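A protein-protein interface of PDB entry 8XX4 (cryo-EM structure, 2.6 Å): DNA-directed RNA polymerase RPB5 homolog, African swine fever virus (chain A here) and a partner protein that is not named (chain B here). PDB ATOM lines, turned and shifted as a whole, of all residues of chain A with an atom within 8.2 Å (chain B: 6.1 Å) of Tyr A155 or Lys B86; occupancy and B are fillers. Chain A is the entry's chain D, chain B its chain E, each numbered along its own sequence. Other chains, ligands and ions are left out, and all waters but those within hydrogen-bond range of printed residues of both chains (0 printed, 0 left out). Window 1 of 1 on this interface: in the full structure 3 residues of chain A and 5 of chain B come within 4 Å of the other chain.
NZ of Lys B86 sits at hydrogen-bond distance from OE1 of Gln A157 (3.1 Å). The backbone carbonyl oxygen (O) of Tyr A155 is in hydrogen-bond range of the side-chain amino group (NZ) of Lys B86 (3.0 Å).
The backbone carbonyl oxygen (O) of Ile B94 is in hydrogen-bond range of the backbone NH (N) of Ile B85 (2.8 Å). N of Ile B22 sits at hydrogen-bond distance from O of Val B95 (2.8 Å). O of Lys B86 sits at hydrogen-bond distance from N of Ile B94, 2.9 Å away.
Among the printed residues, merely in contact across the chains: Tyr A155 with Ile B22 (3.8 Å), Tyr A155 with Ile B85 (3.7 Å) and Tyr A155 with Ile B94 (3.9 Å).
Of the printed residues of chain B, Tyr A155 touches Ile B22, Ile B85, Lys B86 and Ile B94. Printed residues of chain B within 4 Å of Gln A157: Lys B86 (3.1 Å). Cys B84 touches none of the printed residues of chain A. Of the printed residues of chain A, Ile B85 touches Tyr A155 (3.7 Å). Of chain A, only Tyr A155 (3.0 Å) and Gln A157 (3.1 Å) come within 4 Å of Lys B86. The nearest residue of chain B that does not touch Tyr A155 is Glu B96 (5.9 Å). The nearest residue of chain A that does not touch Lys B86 is Leu A156 (4.3 Å).
Printed residues of chain B that touch a printed residue of chain A: Ile B22, Ile B85, Lys B86 and Ile B94. Printed residues of chain A that touch a printed residue of chain B: Tyr A155 and Gln A157. Hydrophobic or aromatic side chains of chain A that line the printed part of chain B: Tyr A155. Among the printed residues, 5 pairs touch across the chains.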
ATOM      1  N   GLN A 148       1.467  21.161   8.305  1.00  0.00           N
ATOM      2  CA  GLN A 148       2.508  20.761   9.245  1.00  0.00           C
ATOM      3  C   GLN A 148       3.772  20.329   8.522  1.00  0.00           C
ATOM      4  O   GLN A 148       4.879  20.662   8.950  1.00  0.00           O
ATOM      5  CB  GLN A 148       2.005  19.642  10.155  1.00  0.00           C
ATOM      6  CG  GLN A 148       1.346  20.124  11.437  1.00  0.00           C
ATOM      7  CD  GLN A 148       1.812  21.505  11.852  1.00  0.00           C
ATOM      8  OE1 GLN A 148       2.959  21.693  12.253  1.00  0.00           O
ATOM      9  NE2 GLN A 148       0.918  22.482  11.761  1.00  0.00           N
ATOM     10  N   GLU A 149       3.634  19.584   7.426  1.00  0.00           N
ATOM     11  CA  GLU A 149       4.834  19.180   6.703  1.00  0.00           C
ATOM     12  C   GLU A 149       5.483  20.364   5.994  1.00  0.00           C
ATOM     13  O   GLU A 149       6.716  20.434   5.912  1.00  0.00           O
ATOM     14  CB  GLU A 149       4.517  18.045   5.726  1.00  0.00           C
ATOM     15  CG  GLU A 149       3.666  18.420   4.543  1.00  0.00           C
ATOM     16  CD  GLU A 149       4.484  18.619   3.290  1.00  0.00           C
ATOM     17  OE1 GLU A 149       5.615  18.092   3.235  1.00  0.00           O
ATOM     18  OE2 GLU A 149       3.999  19.302   2.361  1.00  0.00           O
ATOM     19  N   PHE A 150       4.684  21.316   5.503  1.00  0.00           N
ATOM     20  CA  PHE A 150       5.253  22.529   4.925  1.00  0.00           C
ATOM     21  C   PHE A 150       6.025  23.322   5.971  1.00  0.00           C
ATOM     22  O   PHE A 150       7.131  23.803   5.711  1.00  0.00           O
ATOM     23  CB  PHE A 150       4.147  23.386   4.307  1.00  0.00           C
ATOM     24  CG  PHE A 150       4.548  24.815   4.066  1.00  0.00           C
ATOM     25  CD1 PHE A 150       5.374  25.147   3.010  1.00  0.00           C
ATOM     26  CD2 PHE A 150       4.092  25.825   4.889  1.00  0.00           C
ATOM     27  CE1 PHE A 150       5.739  26.454   2.785  1.00  0.00           C
ATOM     28  CE2 PHE A 150       4.460  27.133   4.667  1.00  0.00           C
ATOM     29  CZ  PHE A 150       5.283  27.445   3.615  1.00  0.00           C
ATOM     30  N   LEU A 151       5.455  23.468   7.167  1.00  0.00           N
ATOM     31  CA  LEU A 151       6.118  24.227   8.219  1.00  0.00           C
ATOM     32  C   LEU A 151       7.360  23.507   8.719  1.00  0.00           C
ATOM     33  O   LEU A 151       8.362  24.146   9.051  1.00  0.00           O
ATOM     34  CB  LEU A 151       5.153  24.484   9.374  1.00  0.00           C
ATOM     35  CG  LEU A 151       3.930  25.357   9.106  1.00  0.00           C
ATOM     36  CD1 LEU A 151       2.977  25.258  10.268  1.00  0.00           C
ATOM     37  CD2 LEU A 151       4.330  26.791   8.876  1.00  0.00           C
ATOM     38  N   GLY A 152       7.311  22.178   8.792  1.00  0.00           N
ATOM     39  CA  GLY A 152       8.479  21.428   9.207  1.00  0.00           C
ATOM     40  C   GLY A 152       9.612  21.523   8.210  1.00  0.00           C
ATOM     41  O   GLY A 152      10.779  21.618   8.594  1.00  0.00           O
ATOM     42  N   ARG A 153       9.290  21.491   6.916  1.00  0.00           N
ATOM     43  CA  ARG A 153      10.324  21.679   5.907  1.00  0.00           C
ATOM     44  C   ARG A 153      10.923  23.075   5.985  1.00  0.00           C
ATOM     45  O   ARG A 153      12.133  23.252   5.807  1.00  0.00           O
ATOM     46  CB  ARG A 153       9.755  21.421   4.516  1.00  0.00           C
ATOM     47  CG  ARG A 153      10.809  21.242   3.455  1.00  0.00           C
ATOM     48  CD  ARG A 153      10.713  22.320   2.408  1.00  0.00           C
ATOM     49  NE  ARG A 153      11.932  22.420   1.619  1.00  0.00           N
ATOM     50  CZ  ARG A 153      12.419  23.556   1.144  1.00  0.00           C
ATOM     51  NH1 ARG A 153      11.805  24.707   1.349  1.00  0.00           N
ATOM     52  NH2 ARG A 153      13.546  23.534   0.441  1.00  0.00           N
ATOM     53  N   GLU A 154      10.095  24.080   6.254  1.00  0.00           N
ATOM     54  CA  GLU A 154      10.526  25.467   6.297  1.00  0.00           C
ATOM     55  C   GLU A 154      11.013  25.905   7.669  1.00  0.00           C
ATOM     56  O   GLU A 154      11.434  27.055   7.815  1.00  0.00           O
ATOM     57  CB  GLU A 154       9.389  26.385   5.849  1.00  0.00           C
ATOM     58  CG  GLU A 154       8.889  26.118   4.454  1.00  0.00           C
ATOM     59  CD  GLU A 154       9.745  26.773   3.402  1.00  0.00           C
ATOM     60  OE1 GLU A 154      10.122  27.944   3.592  1.00  0.00           O
ATOM     61  OE2 GLU A 154      10.045  26.117   2.386  1.00  0.00           O
ATOM     62  N   TYR A 155      10.968  25.025   8.669  1.00  0.00           N
ATOM     63  CA  TYR A 155      11.375  25.358  10.035  1.00  0.00           C
ATOM     64  C   TYR A 155      10.623  26.579  10.547  1.00  0.00           C
ATOM     65  O   TYR A 155      11.193  27.472  11.174  1.00  0.00           O
ATOM     66  CB  TYR A 155      12.885  25.574  10.128  1.00  0.00           C
ATOM     67  CG  TYR A 155      13.666  24.304  10.321  1.00  0.00           C
ATOM     68  CD1 TYR A 155      13.699  23.670  11.550  1.00  0.00           C
ATOM     69  CD2 TYR A 155      14.364  23.734   9.273  1.00  0.00           C
ATOM     70  CE1 TYR A 155      14.409  22.507  11.727  1.00  0.00           C
ATOM     71  CE2 TYR A 155      15.075  22.574   9.442  1.00  0.00           C
ATOM     72  CZ  TYR A 155      15.095  21.964  10.668  1.00  0.00           C
ATOM     73  OH  TYR A 155      15.807  20.803  10.836  1.00  0.00           O
ATOM     74  N   LEU A 156       9.325  26.616  10.276  1.00  0.00           N
ATOM     75  CA  LEU A 156       8.490  27.754  10.611  1.00  0.00           C
ATOM     76  C   LEU A 156       7.455  27.356  11.650  1.00  0.00           C
ATOM     77  O   LEU A 156       7.088  26.187  11.771  1.00  0.00           O
ATOM     78  CB  LEU A 156       7.773  28.303   9.374  1.00  0.00           C
ATOM     79  CG  LEU A 156       8.566  29.148   8.383  1.00  0.00           C
ATOM     80  CD1 LEU A 156       7.735  29.385   7.150  1.00  0.00           C
ATOM     81  CD2 LEU A 156       8.983  30.458   9.003  1.00  0.00           C
ATOM     82  N   GLN A 157       7.021  28.312  12.382  1.00  0.00           N
ATOM     83  CA  GLN A 157       5.853  28.224  13.233  1.00  0.00           C
ATOM     84  C   GLN A 157       4.664  28.863  12.530  1.00  0.00           C
ATOM     85  O   GLN A 157       4.843  29.714  11.657  1.00  0.00           O
ATOM     86  CB  GLN A 157       6.096  28.927  14.570  1.00  0.00           C
ATOM     87  CG  GLN A 157       7.387  28.529  15.254  1.00  0.00           C
ATOM     88  CD  GLN A 157       7.413  27.064  15.634  1.00  0.00           C
ATOM     89  OE1 GLN A 157       8.430  26.389  15.481  1.00  0.00           O
ATOM     90  NE2 GLN A 157       6.293  26.563  16.136  1.00  0.00           N
ATOM     91  N   PRO A 158       3.436  28.463  12.863  1.00  0.00           N
ATOM     92  CA  PRO A 158       2.273  29.096  12.224  1.00  0.00           C
ATOM     93  C   PRO A 158       2.221  30.597  12.426  1.00  0.00           C
ATOM     94  O   PRO A 158       1.688  31.314  11.572  1.00  0.00           O
ATOM     95  CB  PRO A 158       1.089  28.390  12.890  1.00  0.00           C
ATOM     96  CG  PRO A 158       1.626  27.077  13.298  1.00  0.00           C
ATOM     97  CD  PRO A 158       3.048  27.310  13.690  1.00  0.00           C
ATOM     98  N   ASP A 160       4.725  32.569  12.301  1.00  0.00           N
ATOM     99  CA  ASP A 160       5.695  33.192  11.415  1.00  0.00           C
ATOM    100  C   ASP A 160       5.156  33.425  10.014  1.00  0.00           C
ATOM    101  O   ASP A 160       5.776  34.166   9.248  1.00  0.00           O
ATOM    102  CB  ASP A 160       6.958  32.335  11.336  1.00  0.00           C
ATOM    103  CG  ASP A 160       7.679  32.228  12.666  1.00  0.00           C
ATOM    104  OD1 ASP A 160       7.218  32.845  13.647  1.00  0.00           O
ATOM    105  OD2 ASP A 160       8.714  31.533  12.730  1.00  0.00           O
ATOM    106  N   ILE B  22      22.442  20.188  11.278  1.00  0.00           N
ATOM    107  CA  ILE B  22      21.620  19.447  10.316  1.00  0.00           C
ATOM    108  C   ILE B  22      22.509  18.491   9.536  1.00  0.00           C
ATOM    109  O   ILE B  22      23.591  18.897   9.078  1.00  0.00           O
ATOM    110  CB  ILE B  22      20.900  20.421   9.383  1.00  0.00           C
ATOM    111  CG1 ILE B  22      19.733  21.082  10.110  1.00  0.00           C
ATOM    112  CG2 ILE B  22      20.407  19.717   8.143  1.00  0.00           C
ATOM    113  CD1 ILE B  22      19.006  22.099   9.282  1.00  0.00           C
ATOM    114  N   ARG B  83      25.259  28.231   8.816  1.00  0.00           N
ATOM    115  CA  ARG B  83      24.022  28.931   8.503  1.00  0.00           C
ATOM    116  C   ARG B  83      22.986  28.554   9.549  1.00  0.00           C
ATOM    117  O   ARG B  83      22.481  27.430   9.549  1.00  0.00           O
ATOM    118  CB  ARG B  83      23.548  28.576   7.098  1.00  0.00           C
ATOM    119  CG  ARG B  83      24.575  28.850   6.026  1.00  0.00           C
ATOM    120  CD  ARG B  83      24.075  28.421   4.671  1.00  0.00           C
ATOM    121  NE  ARG B  83      24.778  29.090   3.588  1.00  0.00           N
ATOM    122  CZ  ARG B  83      24.938  28.582   2.377  1.00  0.00           C
ATOM    123  NH1 ARG B  83      24.480  27.384   2.067  1.00  0.00           N
ATOM    124  NH2 ARG B  83      25.573  29.294   1.453  1.00  0.00           N
ATOM    125  N   CYS B  84      22.673  29.490  10.439  1.00  0.00           N
ATOM    126  CA  CYS B  84      21.714  29.244  11.507  1.00  0.00           C
ATOM    127  C   CYS B  84      20.310  29.304  10.928  1.00  0.00           C
ATOM    128  O   CYS B  84      19.842  30.369  10.520  1.00  0.00           O
ATOM    129  CB  CYS B  84      21.892  30.259  12.630  1.00  0.00           C
ATOM    130  SG  CYS B  84      20.775  30.028  14.030  1.00  0.00           S
ATOM    131  N   ILE B  85      19.630  28.162  10.900  1.00  0.00           N
ATOM    132  CA  ILE B  85      18.320  28.057  10.274  1.00  0.00           C
ATOM    133  C   ILE B  85      17.239  28.474  11.258  1.00  0.00           C
ATOM    134  O   ILE B  85      16.432  29.363  10.972  1.00  0.00           O
ATOM    135  CB  ILE B  85      18.071  26.627   9.765  1.00  0.00           C
ATOM    136  CG1 ILE B  85      19.208  26.184   8.850  1.00  0.00           C
ATOM    137  CG2 ILE B  85      16.739  26.544   9.056  1.00  0.00           C
ATOM    138  CD1 ILE B  85      19.473  27.127   7.713  1.00  0.00           C
ATOM    139  N   LYS B  86      17.218  27.836  12.424  1.00  0.00           N
ATOM    140  CA  LYS B  86      16.150  28.019  13.389  1.00  0.00           C
ATOM    141  C   LYS B  86      16.736  28.075  14.788  1.00  0.00           C
ATOM    142  O   LYS B  86      17.796  27.509  15.057  1.00  0.00           O
ATOM    143  CB  LYS B  86      15.118  26.886  13.289  1.00  0.00           C
ATOM    144  CG  LYS B  86      13.853  27.087  14.096  1.00  0.00           C
ATOM    145  CD  LYS B  86      13.269  28.463  13.875  1.00  0.00           C
ATOM    146  CE  LYS B  86      11.812  28.513  14.294  1.00  0.00           C
ATOM    147  NZ  LYS B  86      11.156  27.187  14.154  1.00  0.00           N
ATOM    148  N   VAL B  87      16.039  28.772  15.675  1.00  0.00           N
ATOM    149  CA  VAL B  87      16.345  28.776  17.101  1.00  0.00           C
ATOM    150  C   VAL B  87      15.126  28.186  17.801  1.00  0.00           C
ATOM    151  O   VAL B  87      14.167  28.889  18.125  1.00  0.00           O
ATOM    152  CB  VAL B  87      16.680  30.171  17.628  1.00  0.00           C
ATOM    153  CG1 VAL B  87      17.487  30.057  18.893  1.00  0.00           C
ATOM    154  CG2 VAL B  87      17.444  30.959  16.586  1.00  0.00           C
ATOM    155  N   THR B  88      15.161  26.881  18.024  1.00  0.00           N
ATOM    156  CA  THR B  88      14.089  26.198  18.730  1.00  0.00           C
ATOM    157  C   THR B  88      13.986  26.729  20.158  1.00  0.00           C
ATOM    158  O   THR B  88      15.013  26.927  20.818  1.00  0.00           O
ATOM    159  CB  THR B  88      14.371  24.692  18.718  1.00  0.00           C
ATOM    160  OG1 THR B  88      13.882  24.121  17.497  1.00  0.00           O
ATOM    161  CG2 THR B  88      13.758  23.975  19.896  1.00  0.00           C
ATOM    162  N   GLN B  92      17.591  24.861  21.421  1.00  0.00           N
ATOM    163  CA  GLN B  92      18.299  24.218  20.325  1.00  0.00           C
ATOM    164  C   GLN B  92      18.556  25.223  19.215  1.00  0.00           C
ATOM    165  O   GLN B  92      17.637  25.909  18.763  1.00  0.00           O
ATOM    166  CB  GLN B  92      17.495  23.038  19.782  1.00  0.00           C
ATOM    167  CG  GLN B  92      17.321  21.905  20.772  1.00  0.00           C
ATOM    168  CD  GLN B  92      17.347  20.547  20.112  1.00  0.00           C
ATOM    169  OE1 GLN B  92      16.787  20.359  19.033  1.00  0.00           O
ATOM    170  NE2 GLN B  92      17.999  19.587  20.756  1.00  0.00           N
ATOM    171  N   LYS B  93      19.805  25.306  18.777  1.00  0.00           N
ATOM    172  CA  LYS B  93      20.196  26.172  17.669  1.00  0.00           C
ATOM    173  C   LYS B  93      20.457  25.276  16.468  1.00  0.00           C
ATOM    174  O   LYS B  93      21.479  24.590  16.404  1.00  0.00           O
ATOM    175  CB  LYS B  93      21.419  27.007  18.023  1.00  0.00           C
ATOM    176  CG  LYS B  93      21.760  28.049  16.981  1.00  0.00           C
ATOM    177  CD  LYS B  93      22.398  29.267  17.605  1.00  0.00           C
ATOM    178  CE  LYS B  93      23.785  29.499  17.049  1.00  0.00           C
ATOM    179  NZ  LYS B  93      23.745  30.316  15.810  1.00  0.00           N
ATOM    180  N   ILE B  94      19.528  25.282  15.520  1.00  0.00           N
ATOM    181  CA  ILE B  94      19.612  24.417  14.350  1.00  0.00           C
ATOM    182  C   ILE B  94      20.405  25.138  13.268  1.00  0.00           C
ATOM    183  O   ILE B  94      20.013  26.215  12.814  1.00  0.00           O
ATOM    184  CB  ILE B  94      18.214  24.033  13.853  1.00  0.00           C
ATOM    185  CG1 ILE B  94      17.511  23.153  14.881  1.00  0.00           C
ATOM    186  CG2 ILE B  94      18.300  23.323  12.532  1.00  0.00           C
ATOM    187  CD1 ILE B  94      16.116  23.600  15.194  1.00  0.00           C
ATOM    188  N   VAL B  95      21.523  24.544  12.853  1.00  0.00           N
ATOM    189  CA  VAL B  95      22.422  25.165  11.894  1.00  0.00           C
ATOM    190  C   VAL B  95      22.733  24.184  10.775  1.00  0.00           C
ATOM    191  O   VAL B  95      22.540  22.974  10.900  1.00  0.00           O
ATOM    192  CB  VAL B  95      23.736  25.648  12.545  1.00  0.00           C
ATOM    193  CG1 VAL B  95      23.450  26.577  13.701  1.00  0.00           C
ATOM    194  CG2 VAL B  95      24.566  24.466  12.994  1.00  0.00           C
ATOM    195  N   GLU B  96      23.211  24.732   9.663  1.00  0.00           N
ATOM    196  CA  GLU B  96      23.759  23.959   8.560  1.00  0.00           C
ATOM    197  C   GLU B  96      25.207  24.376   8.375  1.00  0.00           C
ATOM    198  O   GLU B  96      25.483  25.538   8.066  1.00  0.00           O
ATOM    199  CB  GLU B  96      22.970  24.188   7.273  1.00  0.00           C
ATOM    200  CG  GLU B  96      21.594  23.579   7.284  1.00  0.00           C
ATOM    201  CD  GLU B  96      20.883  23.729   5.964  1.00  0.00           C
ATOM    202  OE1 GLU B  96      21.542  24.118   4.982  1.00  0.00           O
ATOM    203  OE2 GLU B  96      19.667  23.458   5.908  1.00  0.00           O
